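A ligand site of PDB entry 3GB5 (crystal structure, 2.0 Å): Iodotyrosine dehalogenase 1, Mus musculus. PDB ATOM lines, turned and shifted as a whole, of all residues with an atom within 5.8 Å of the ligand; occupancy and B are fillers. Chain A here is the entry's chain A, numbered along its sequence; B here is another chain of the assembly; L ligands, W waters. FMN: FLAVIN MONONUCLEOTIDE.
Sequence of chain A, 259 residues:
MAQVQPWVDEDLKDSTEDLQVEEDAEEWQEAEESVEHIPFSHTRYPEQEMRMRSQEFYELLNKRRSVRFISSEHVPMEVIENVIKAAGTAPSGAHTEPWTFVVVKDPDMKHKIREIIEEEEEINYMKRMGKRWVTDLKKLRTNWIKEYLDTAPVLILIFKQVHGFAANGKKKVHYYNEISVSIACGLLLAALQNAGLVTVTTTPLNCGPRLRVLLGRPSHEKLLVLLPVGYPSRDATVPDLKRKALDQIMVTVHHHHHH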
ATOM      1  N   ARG A  64      24.715   6.482  28.448  1.00  0.00           N
ATOM      2  CA  ARG A  64      24.285   5.398  27.545  1.00  0.00           C
ATOM      3  C   ARG A  64      24.659   4.008  28.142  1.00  0.00           C
ATOM      4  O   ARG A  64      25.781   3.794  28.532  1.00  0.00           O
ATOM      5  CB  ARG A  64      24.938   5.559  26.160  1.00  0.00           C
ATOM      6  CG  ARG A  64      24.480   4.450  25.130  1.00  0.00           C
ATOM      7  CD  ARG A  64      25.558   4.143  24.012  1.00  0.00           C
ATOM      8  NE  ARG A  64      26.746   3.595  24.674  1.00  0.00           N
ATOM      9  CZ  ARG A  64      26.841   2.376  25.206  1.00  0.00           C
ATOM     10  NH1 ARG A  64      25.802   1.496  25.143  1.00  0.00           N
ATOM     11  NH2 ARG A  64      27.974   2.041  25.845  1.00  0.00           N
ATOM     12  N   ARG A  65      23.702   3.088  28.219  1.00  0.00           N
ATOM     13  CA  ARG A  65      24.013   1.688  28.592  1.00  0.00           C
ATOM     14  C   ARG A  65      23.282   0.786  27.596  1.00  0.00           C
ATOM     15  O   ARG A  65      22.205   1.154  27.104  1.00  0.00           O
ATOM     16  CB  ARG A  65      23.572   1.330  30.031  1.00  0.00           C
ATOM     17  CG  ARG A  65      24.330   2.083  31.181  1.00  0.00           C
ATOM     18  CD  ARG A  65      25.853   1.782  31.166  1.00  0.00           C
ATOM     19  NE  ARG A  65      26.085   0.337  31.215  1.00  0.00           N
ATOM     20  CZ  ARG A  65      26.121  -0.382  32.329  1.00  0.00           C
ATOM     21  NH1 ARG A  65      25.972   0.210  33.529  1.00  0.00           N
ATOM     22  NH2 ARG A  65      26.335  -1.700  32.252  1.00  0.00           N
ATOM     23  N   SER A  66      23.862  -0.392  27.312  1.00  0.00           N
ATOM     24  CA  SER A  66      23.158  -1.414  26.545  1.00  0.00           C
ATOM     25  C   SER A  66      22.020  -1.958  27.389  1.00  0.00           C
ATOM     26  O   SER A  66      22.234  -2.394  28.519  1.00  0.00           O
ATOM     27  CB  SER A  66      24.097  -2.574  26.130  1.00  0.00           C
ATOM     28  OG  SER A  66      25.083  -2.074  25.210  1.00  0.00           O
ATOM     29  N   ARG A  68      18.766  -4.564  27.699  1.00  0.00           N
ATOM     30  CA  ARG A  68      18.239  -5.774  27.043  1.00  0.00           C
ATOM     31  C   ARG A  68      16.781  -6.032  27.437  1.00  0.00           C
ATOM     32  O   ARG A  68      16.260  -7.150  27.229  1.00  0.00           O
ATOM     33  CB  ARG A  68      19.133  -6.993  27.366  1.00  0.00           C
ATOM     34  CG  ARG A  68      20.580  -6.814  26.814  1.00  0.00           C
ATOM     35  CD  ARG A  68      21.589  -7.827  27.400  1.00  0.00           C
ATOM     36  NE  ARG A  68      22.936  -7.553  26.834  1.00  0.00           N
ATOM     37  CZ  ARG A  68      23.835  -6.747  27.406  1.00  0.00           C
ATOM     38  NH1 ARG A  68      23.584  -6.157  28.584  1.00  0.00           N
ATOM     39  NH2 ARG A  68      25.019  -6.562  26.803  1.00  0.00           N
ATOM     40  N   LYS A 146      16.562 -13.322  24.307  1.00  0.00           N
ATOM     41  CA  LYS A 146      16.399 -12.478  23.109  1.00  0.00           C
ATOM     42  C   LYS A 146      14.979 -12.014  22.893  1.00  0.00           C
ATOM     43  O   LYS A 146      14.557 -11.672  21.770  1.00  0.00           O
ATOM     44  CB  LYS A 146      16.863 -13.218  21.861  1.00  0.00           C
ATOM     45  CG  LYS A 146      18.097 -12.679  21.258  1.00  0.00           C
ATOM     46  CD  LYS A 146      19.302 -13.165  22.002  1.00  0.00           C
ATOM     47  CE  LYS A 146      19.974 -14.275  21.222  1.00  0.00           C
ATOM     48  NZ  LYS A 146      21.453 -14.058  21.168  1.00  0.00           N
ATOM     49  N   TYR A 148      13.754  -9.242  23.684  1.00  0.00           N
ATOM     50  CA  TYR A 148      13.715  -7.853  23.239  1.00  0.00           C
ATOM     51  C   TYR A 148      13.548  -7.704  21.710  1.00  0.00           C
ATOM     52  O   TYR A 148      13.135  -6.640  21.221  1.00  0.00           O
ATOM     53  CB  TYR A 148      14.950  -7.083  23.749  1.00  0.00           C
ATOM     54  CG  TYR A 148      16.286  -7.701  23.342  1.00  0.00           C
ATOM     55  CD1 TYR A 148      17.077  -8.387  24.291  1.00  0.00           C
ATOM     56  CD2 TYR A 148      16.742  -7.662  22.014  1.00  0.00           C
ATOM     57  CE1 TYR A 148      18.298  -8.980  23.943  1.00  0.00           C
ATOM     58  CE2 TYR A 148      17.960  -8.257  21.636  1.00  0.00           C
ATOM     59  CZ  TYR A 148      18.734  -8.892  22.618  1.00  0.00           C
ATOM     60  OH  TYR A 148      19.929  -9.454  22.281  1.00  0.00           O
ATOM     61  N   VAL A 200      20.481  -2.362  22.441  1.00  0.00           N
ATOM     62  CA  VAL A 200      21.661  -3.163  22.745  1.00  0.00           C
ATOM     63  C   VAL A 200      22.308  -3.450  21.378  1.00  0.00           C
ATOM     64  O   VAL A 200      21.694  -4.030  20.466  1.00  0.00           O
ATOM     65  CB  VAL A 200      21.364  -4.476  23.589  1.00  0.00           C
ATOM     66  CG1 VAL A 200      20.129  -5.271  23.046  1.00  0.00           C
ATOM     67  CG2 VAL A 200      22.618  -5.399  23.687  1.00  0.00           C
ATOM     68  N   THR A 201      23.553  -3.033  21.235  1.00  0.00           N
ATOM     69  CA  THR A 201      24.322  -3.347  20.023  1.00  0.00           C
ATOM     70  C   THR A 201      24.521  -4.871  19.915  1.00  0.00           C
ATOM     71  O   THR A 201      25.069  -5.526  20.844  1.00  0.00           O
ATOM     72  CB  THR A 201      25.697  -2.613  20.034  1.00  0.00           C
ATOM     73  OG1 THR A 201      25.456  -1.227  20.125  1.00  0.00           O
ATOM     74  CG2 THR A 201      26.492  -2.918  18.774  1.00  0.00           C
ATOM     75  N   THR A 202      24.083  -5.442  18.784  1.00  0.00           N
ATOM     76  CA  THR A 202      24.439  -6.837  18.485  1.00  0.00           C
ATOM     77  C   THR A 202      24.955  -6.951  17.056  1.00  0.00           C
ATOM     78  O   THR A 202      24.623  -6.137  16.199  1.00  0.00           O
ATOM     79  CB  THR A 202      23.240  -7.848  18.665  1.00  0.00           C
ATOM     80  OG1 THR A 202      22.277  -7.623  17.619  1.00  0.00           O
ATOM     81  CG2 THR A 202      22.598  -7.658  20.041  1.00  0.00           C
ATOM     82  N   THR A 203      25.812  -7.944  16.838  1.00  0.00           N
ATOM     83  CA  THR A 203      26.411  -8.132  15.511  1.00  0.00           C
ATOM     84  C   THR A 203      26.262  -9.596  15.115  1.00  0.00           C
ATOM     85  O   THR A 203      27.238 -10.337  15.198  1.00  0.00           O
ATOM     86  CB  THR A 203      27.929  -7.710  15.470  1.00  0.00           C
ATOM     87  OG1 THR A 203      28.643  -8.420  16.487  1.00  0.00           O
ATOM     88  CG2 THR A 203      28.100  -6.225  15.677  1.00  0.00           C
ATOM     89  N   VAL A 238      20.715  -3.334  34.281  1.00  0.00           N
ATOM     90  CA  VAL A 238      21.949  -3.447  33.502  1.00  0.00           C
ATOM     91  C   VAL A 238      23.001  -4.101  34.422  1.00  0.00           C
ATOM     92  O   VAL A 238      22.885  -3.988  35.659  1.00  0.00           O
ATOM     93  CB  VAL A 238      22.473  -2.051  32.986  1.00  0.00           C
ATOM     94  CG1 VAL A 238      21.519  -1.441  31.890  1.00  0.00           C
ATOM     95  CG2 VAL A 238      22.666  -1.108  34.168  1.00  0.00           C
ATOM     96  N   PRO A 239      24.004  -4.808  33.847  1.00  0.00           N
ATOM     97  CA  PRO A 239      25.059  -5.293  34.763  1.00  0.00           C
ATOM     98  C   PRO A 239      25.840  -4.099  35.322  1.00  0.00           C
ATOM     99  O   PRO A 239      25.947  -3.055  34.655  1.00  0.00           O
ATOM    100  CB  PRO A 239      25.979  -6.146  33.864  1.00  0.00           C
ATOM    101  CG  PRO A 239      25.603  -5.843  32.478  1.00  0.00           C
ATOM    102  CD  PRO A 239      24.248  -5.158  32.447  1.00  0.00           C
ATOM    103  N   LEU A 241      28.694  -2.614  35.459  1.00  0.00           N
ATOM    104  CA  LEU A 241      30.015  -2.460  34.870  1.00  0.00           C
ATOM    105  C   LEU A 241      30.495  -1.042  35.088  1.00  0.00           C
ATOM    106  O   LEU A 241      29.703  -0.095  35.085  1.00  0.00           O
ATOM    107  CB  LEU A 241      29.957  -2.735  33.349  1.00  0.00           C
ATOM    108  CG  LEU A 241      29.291  -4.029  32.860  1.00  0.00           C
ATOM    109  CD1 LEU A 241      29.185  -3.988  31.317  1.00  0.00           C
ATOM    110  CD2 LEU A 241      30.068  -5.279  33.360  1.00  0.00           C
ATOM    111  N   ARG A 243      33.275   1.779  33.480  1.00  0.00           N
ATOM    112  CA  ARG A 243      34.095   2.122  32.336  1.00  0.00           C
ATOM    113  C   ARG A 243      35.528   2.414  32.788  1.00  0.00           C
ATOM    114  O   ARG A 243      35.769   2.786  33.944  1.00  0.00           O
ATOM    115  CB  ARG A 243      33.562   3.350  31.570  1.00  0.00           C
ATOM    116  CG  ARG A 243      32.172   3.164  31.060  1.00  0.00           C
ATOM    117  CD  ARG A 243      31.773   4.061  29.927  1.00  0.00           C
ATOM    118  NE  ARG A 243      30.723   3.302  29.243  1.00  0.00           N
ATOM    119  CZ  ARG A 243      29.448   3.618  29.221  1.00  0.00           C
ATOM    120  NH1 ARG A 243      29.036   4.704  29.834  1.00  0.00           N
ATOM    121  NH2 ARG A 243      28.579   2.843  28.607  1.00  0.00           N
ATOM    122  N   THR B  89      33.104   5.953  25.930  1.00  0.00           N
ATOM    123  CA  THR B  89      31.735   5.543  26.316  1.00  0.00           C
ATOM    124  C   THR B  89      31.144   4.405  25.445  1.00  0.00           C
ATOM    125  O   THR B  89      30.006   4.007  25.732  1.00  0.00           O
ATOM    126  CB  THR B  89      30.726   6.719  26.523  1.00  0.00           C
ATOM    127  OG1 THR B  89      30.429   7.323  25.268  1.00  0.00           O
ATOM    128  CG2 THR B  89      31.276   7.777  27.515  1.00  0.00           C
ATOM    129  N   ALA B  90      31.825   3.950  24.352  1.00  0.00           N
ATOM    130  CA  ALA B  90      31.213   3.284  23.177  1.00  0.00           C
ATOM    131  C   ALA B  90      30.788   1.971  23.934  1.00  0.00           C
ATOM    132  O   ALA B  90      31.540   1.514  24.854  1.00  0.00           O
ATOM    133  CB  ALA B  90      32.253   2.956  22.104  1.00  0.00           C
ATOM    134  N   PRO B  91      29.829   1.170  23.393  1.00  0.00           N
ATOM    135  CA  PRO B  91      29.781  -0.277  23.580  1.00  0.00           C
ATOM    136  C   PRO B  91      30.993  -1.068  23.063  1.00  0.00           C
ATOM    137  O   PRO B  91      31.718  -0.596  22.215  1.00  0.00           O
ATOM    138  CB  PRO B  91      28.467  -0.663  22.898  1.00  0.00           C
ATOM    139  CG  PRO B  91      28.488   0.247  21.634  1.00  0.00           C
ATOM    140  CD  PRO B  91      28.966   1.601  22.256  1.00  0.00           C
ATOM    141  N   SER B  92      31.184  -2.253  23.625  1.00  0.00           N
ATOM    142  CA  SER B  92      32.225  -3.164  23.112  1.00  0.00           C
ATOM    143  C   SER B  92      31.823  -4.591  23.366  1.00  0.00           C
ATOM    144  O   SER B  92      31.314  -4.931  24.466  1.00  0.00           O
ATOM    145  CB  SER B  92      33.622  -2.854  23.721  1.00  0.00           C
ATOM    146  OG  SER B  92      33.673  -3.015  25.147  1.00  0.00           O
ATOM    147  N   GLY B  93      32.147  -5.443  22.383  1.00  0.00           N
ATOM    148  CA  GLY B  93      31.972  -6.882  22.490  1.00  0.00           C
ATOM    149  C   GLY B  93      32.567  -7.430  23.763  1.00  0.00           C
ATOM    150  O   GLY B  93      33.733  -7.183  24.084  1.00  0.00           O
ATOM    151  N   ALA B  94      31.769  -8.169  24.534  1.00  0.00           N
ATOM    152  CA  ALA B  94      32.219  -8.708  25.842  1.00  0.00           C
ATOM    153  C   ALA B  94      32.808  -7.674  26.860  1.00  0.00           C
ATOM    154  O   ALA B  94      33.581  -8.044  27.748  1.00  0.00           O
ATOM    155  CB  ALA B  94      33.132 -10.009  25.670  1.00  0.00           C
ATOM    156  N   HIS B  95      32.426  -6.402  26.718  1.00  0.00           N
ATOM    157  CA  HIS B  95      32.904  -5.307  27.571  1.00  0.00           C
ATOM    158  C   HIS B  95      34.444  -5.372  27.692  1.00  0.00           C
ATOM    159  O   HIS B  95      34.990  -5.345  28.792  1.00  0.00           O
ATOM    160  CB  HIS B  95      32.177  -5.322  28.940  1.00  0.00           C
ATOM    161  CG  HIS B  95      32.668  -4.293  29.923  1.00  0.00           C
ATOM    162  ND1 HIS B  95      32.597  -2.933  29.695  1.00  0.00           N
ATOM    163  CD2 HIS B  95      33.197  -4.432  31.170  1.00  0.00           C
ATOM    164  CE1 HIS B  95      33.076  -2.286  30.743  1.00  0.00           C
ATOM    165  NE2 HIS B  95      33.440  -3.171  31.654  1.00  0.00           N
ATOM    166  N   TYR B 176      34.843  -9.137  17.963  1.00  0.00           N
ATOM    167  CA  TYR B 176      34.297  -7.970  17.305  1.00  0.00           C
ATOM    168  C   TYR B 176      35.039  -6.668  17.715  1.00  0.00           C
ATOM    169  O   TYR B 176      34.415  -5.619  17.827  1.00  0.00           O
ATOM    170  CB  TYR B 176      32.782  -7.867  17.587  1.00  0.00           C
ATOM    171  CG  TYR B 176      32.012  -9.104  17.147  1.00  0.00           C
ATOM    172  CD1 TYR B 176      31.982  -9.482  15.788  1.00  0.00           C
ATOM    173  CD2 TYR B 176      31.311  -9.893  18.071  1.00  0.00           C
ATOM    174  CE1 TYR B 176      31.299 -10.626  15.352  1.00  0.00           C
ATOM    175  CE2 TYR B 176      30.601 -11.059  17.633  1.00  0.00           C
ATOM    176  CZ  TYR B 176      30.604 -11.412  16.255  1.00  0.00           C
ATOM    177  OH  TYR B 176      29.953 -12.542  15.750  1.00  0.00           O
ATOM    178  N   ILE B 179      34.896  -3.726  14.994  1.00  0.00           N
ATOM    179  CA  ILE B 179      33.615  -3.015  14.989  1.00  0.00           C
ATOM    180  C   ILE B 179      33.484  -2.151  16.231  1.00  0.00           C
ATOM    181  O   ILE B 179      33.103  -0.985  16.142  1.00  0.00           O
ATOM    182  CB  ILE B 179      32.384  -3.985  14.877  1.00  0.00           C
ATOM    183  CG1 ILE B 179      32.357  -4.654  13.498  1.00  0.00           C
ATOM    184  CG2 ILE B 179      31.065  -3.149  15.071  1.00  0.00           C
ATOM    185  CD1 ILE B 179      31.349  -5.833  13.422  1.00  0.00           C
ATOM    186  N   SER B 180      33.838  -2.697  17.408  1.00  0.00           N
ATOM    187  CA  SER B 180      33.719  -1.914  18.687  1.00  0.00           C
ATOM    188  C   SER B 180      34.552  -0.617  18.612  1.00  0.00           C
ATOM    189  O   SER B 180      34.126   0.493  18.969  1.00  0.00           O
ATOM    190  CB  SER B 180      34.154  -2.769  19.894  1.00  0.00           C
ATOM    191  OG  SER B 180      33.399  -3.970  19.971  1.00  0.00           O
ATOM    192  N   ILE B 183      33.128   1.945  16.166  1.00  0.00           N
ATOM    193  CA  ILE B 183      31.971   2.613  16.802  1.00  0.00           C
ATOM    194  C   ILE B 183      32.483   3.749  17.729  1.00  0.00           C
ATOM    195  O   ILE B 183      31.961   4.888  17.703  1.00  0.00           O
ATOM    196  CB  ILE B 183      31.104   1.594  17.594  1.00  0.00           C
ATOM    197  CG1 ILE B 183      30.233   0.741  16.612  1.00  0.00           C
ATOM    198  CG2 ILE B 183      30.162   2.321  18.574  1.00  0.00           C
ATOM    199  CD1 ILE B 183      29.583  -0.554  17.268  1.00  0.00           C
HETATM  200  N1  FMN L   1      25.311  -7.664  23.849  1.00  0.00           N
HETATM  201  C2  FMN L   1      24.506  -8.786  23.829  1.00  0.00           C
HETATM  202  O2  FMN L   1      23.757  -8.959  24.786  1.00  0.00           O
HETATM  203  N3  FMN L   1      24.588  -9.708  22.842  1.00  0.00           N
HETATM  204  C4  FMN L   1      25.448  -9.515  21.804  1.00  0.00           C
HETATM  205  O4  FMN L   1      25.611 -10.424  20.971  1.00  0.00           O
HETATM  206  C4A FMN L   1      26.248  -8.350  21.801  1.00  0.00           C
HETATM  207  N5  FMN L   1      27.114  -8.108  20.749  1.00  0.00           N
HETATM  208  C5A FMN L   1      27.886  -6.944  20.732  1.00  0.00           C
HETATM  209  C6  FMN L   1      28.748  -6.757  19.637  1.00  0.00           C
HETATM  210  C7  FMN L   1      29.509  -5.598  19.531  1.00  0.00           C
HETATM  211  C7M FMN L   1      30.333  -5.393  18.271  1.00  0.00           C
HETATM  212  C8  FMN L   1      29.423  -4.648  20.564  1.00  0.00           C
HETATM  213  C8M FMN L   1      29.927  -3.199  20.387  1.00  0.00           C
HETATM  214  C9  FMN L   1      28.590  -4.872  21.672  1.00  0.00           C
HETATM  215  C9A FMN L   1      27.805  -6.010  21.769  1.00  0.00           C
HETATM  216  N10 FMN L   1      26.946  -6.244  22.843  1.00  0.00           N
HETATM  217  C10 FMN L   1      26.171  -7.418  22.824  1.00  0.00           C
HETATM  218  C1' FMN L   1      26.806  -5.305  23.991  1.00  0.00           C
HETATM  219  C2' FMN L   1      27.982  -5.390  24.973  1.00  0.00           C
HETATM  220  O2' FMN L   1      27.890  -6.542  25.806  1.00  0.00           O
HETATM  221  C3' FMN L   1      28.070  -4.120  25.781  1.00  0.00           C
HETATM  222  O3' FMN L   1      28.377  -2.984  24.967  1.00  0.00           O
HETATM  223  C4' FMN L   1      29.110  -4.231  26.935  1.00  0.00           C
HETATM  224  O4' FMN L   1      28.712  -5.208  27.895  1.00  0.00           O
HETATM  225  C5' FMN L   1      29.270  -2.910  27.641  1.00  0.00           C
HETATM  226  O5' FMN L   1      28.037  -2.442  28.196  1.00  0.00           O
HETATM  227  P   FMN L   1      27.467  -0.986  27.854  1.00  0.00           P
HETATM  228  O1P FMN L   1      26.218  -0.733  28.667  1.00  0.00           O
HETATM  229  O2P FMN L   1      27.124  -0.991  26.355  1.00  0.00           O
HETATM  230  O3P FMN L   1      28.444   0.057  28.201  1.00  0.00           O
HETATM  231  O   HOH W   1      29.205  -8.174  28.763  1.00  0.00           O
HETATM  232  O   HOH W   2      24.814  -2.942  29.698  1.00  0.00           O
HETATM  233  O   HOH W   3      26.537 -10.151  18.552  1.00  0.00           O
HETATM  234  O   HOH W   4      29.970  -0.161  30.259  1.00  0.00           O
HETATM  235  O   HOH W   5      26.366  -9.647  26.915  1.00  0.00           O
HETATM  236  O   HOH W   6      26.315  -5.093  29.053  1.00  0.00           O
HETATM  237  O   HOH W   7      21.463 -10.522  24.217  1.00  0.00           O
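The guanidinium group (NH2) of Arg 243 lies within salt-bridge range of an oxygen (O3P) of the ligand. NH1 of Arg 64 lies within salt-bridge range of O2P of the ligand (3.1 Å). The side-chain hydroxyl of Ser 66 sits at hydrogen-bond distance from an oxygen (O2P) of the ligand (2.6 Å). An oxygen (O1P) of the ligand is in salt-bridge range of the guanidinium group (NE) of Arg 65 (2.8 Å). An oxygen (O2) of the ligand sits at hydrogen-bond distance from the guanidinium group of Arg 68. O1P of the ligand lies within hydrogen-bond range of N of Ser 66 (2.7 Å). The backbone NH (N) of Ser 92 of chain B is in hydrogen-bond range of an oxygen (O3') of the ligand, at 3.2 Å.
The guanidinium group (NH2) of Arg 65 lies within hydrogen-bond range of the backbone carbonyl oxygen (O) of Pro 239. The backbone NH (N) of Gly 93 of chain B lies within hydrogen-bond range of the side-chain hydroxyl (OG) of Ser 180 of chain B. The guanidinium group (NH2) of Arg 243 sits at hydrogen-bond distance from the backbone carbonyl oxygen (O) of Thr 89 of chain B. O of Arg 64 is in hydrogen-bond range of NH2 of Arg 243, at 3.0 Å. The guanidinium group (NH2) of Arg 64 lies within hydrogen-bond range of the backbone carbonyl oxygen (O) of Thr 89 of chain B, 2.8 Å away. The backbone carbonyl oxygen (O) of Tyr 176 of chain B lies within hydrogen-bond range of the side-chain hydroxyl (OG) of Ser 180 of chain B, 2.9 Å away.
The backbone carbonyl oxygen (O) of Thr 201 sits close to a nitrogen (N10) of the ligand (2.8 Å). Residues that only touch the ligand: Val 200 (3.5 Å), Thr 202 (3.7 Å), Thr 203 (3.5 Å), Leu 241 (3.7 Å), Pro 91 of chain B (3.1 Å), Gly 93 of chain B (3.4 Å), His 95 of chain B (3.6 Å), Tyr 176 of chain B (3.5 Å), Ile 179 of chain B (3.98 Å) and Ser 180 of chain B (3.6 Å). Within 4 Å of the ligand: Arg 64, Arg 65, Ser 66, Arg 68, Val 200, Thr 201, Thr 202, Thr 203, Leu 241, Arg 243, Pro 91 of chain B, Ser 92 of chain B, Gly 93 of chain B, His 95 of chain B, Tyr 176 of chain B, Ile 179 of chain B and Ser 180 of chain B. The nearest printed residue that does not touch the ligand is Ile 183 of chain B (4.1 Å).
Water W3 lies within hydrogen-bond range of O4 of the ligand and N of Thr 203. Water W6 bridges O4' of the ligand (2.7 Å) and NH1 of Arg 68 (3.0 Å). Water W2 lies within hydrogen-bond range of an oxygen (O1P) of the ligand (2.8 Å), the backbone carbonyl oxygen of Ser 66 (2.9 Å) and the guanidinium group of Arg 65 (3.2 Å). Water W7 lies within hydrogen-bond range of OH of Tyr 148 (2.7 Å) and O2 of the ligand (2.8 Å). Water W5 bridges the guanidinium group (NH2) of Arg 68 (3.4 Å) and an oxygen (O2) of the ligand (3.4 Å).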
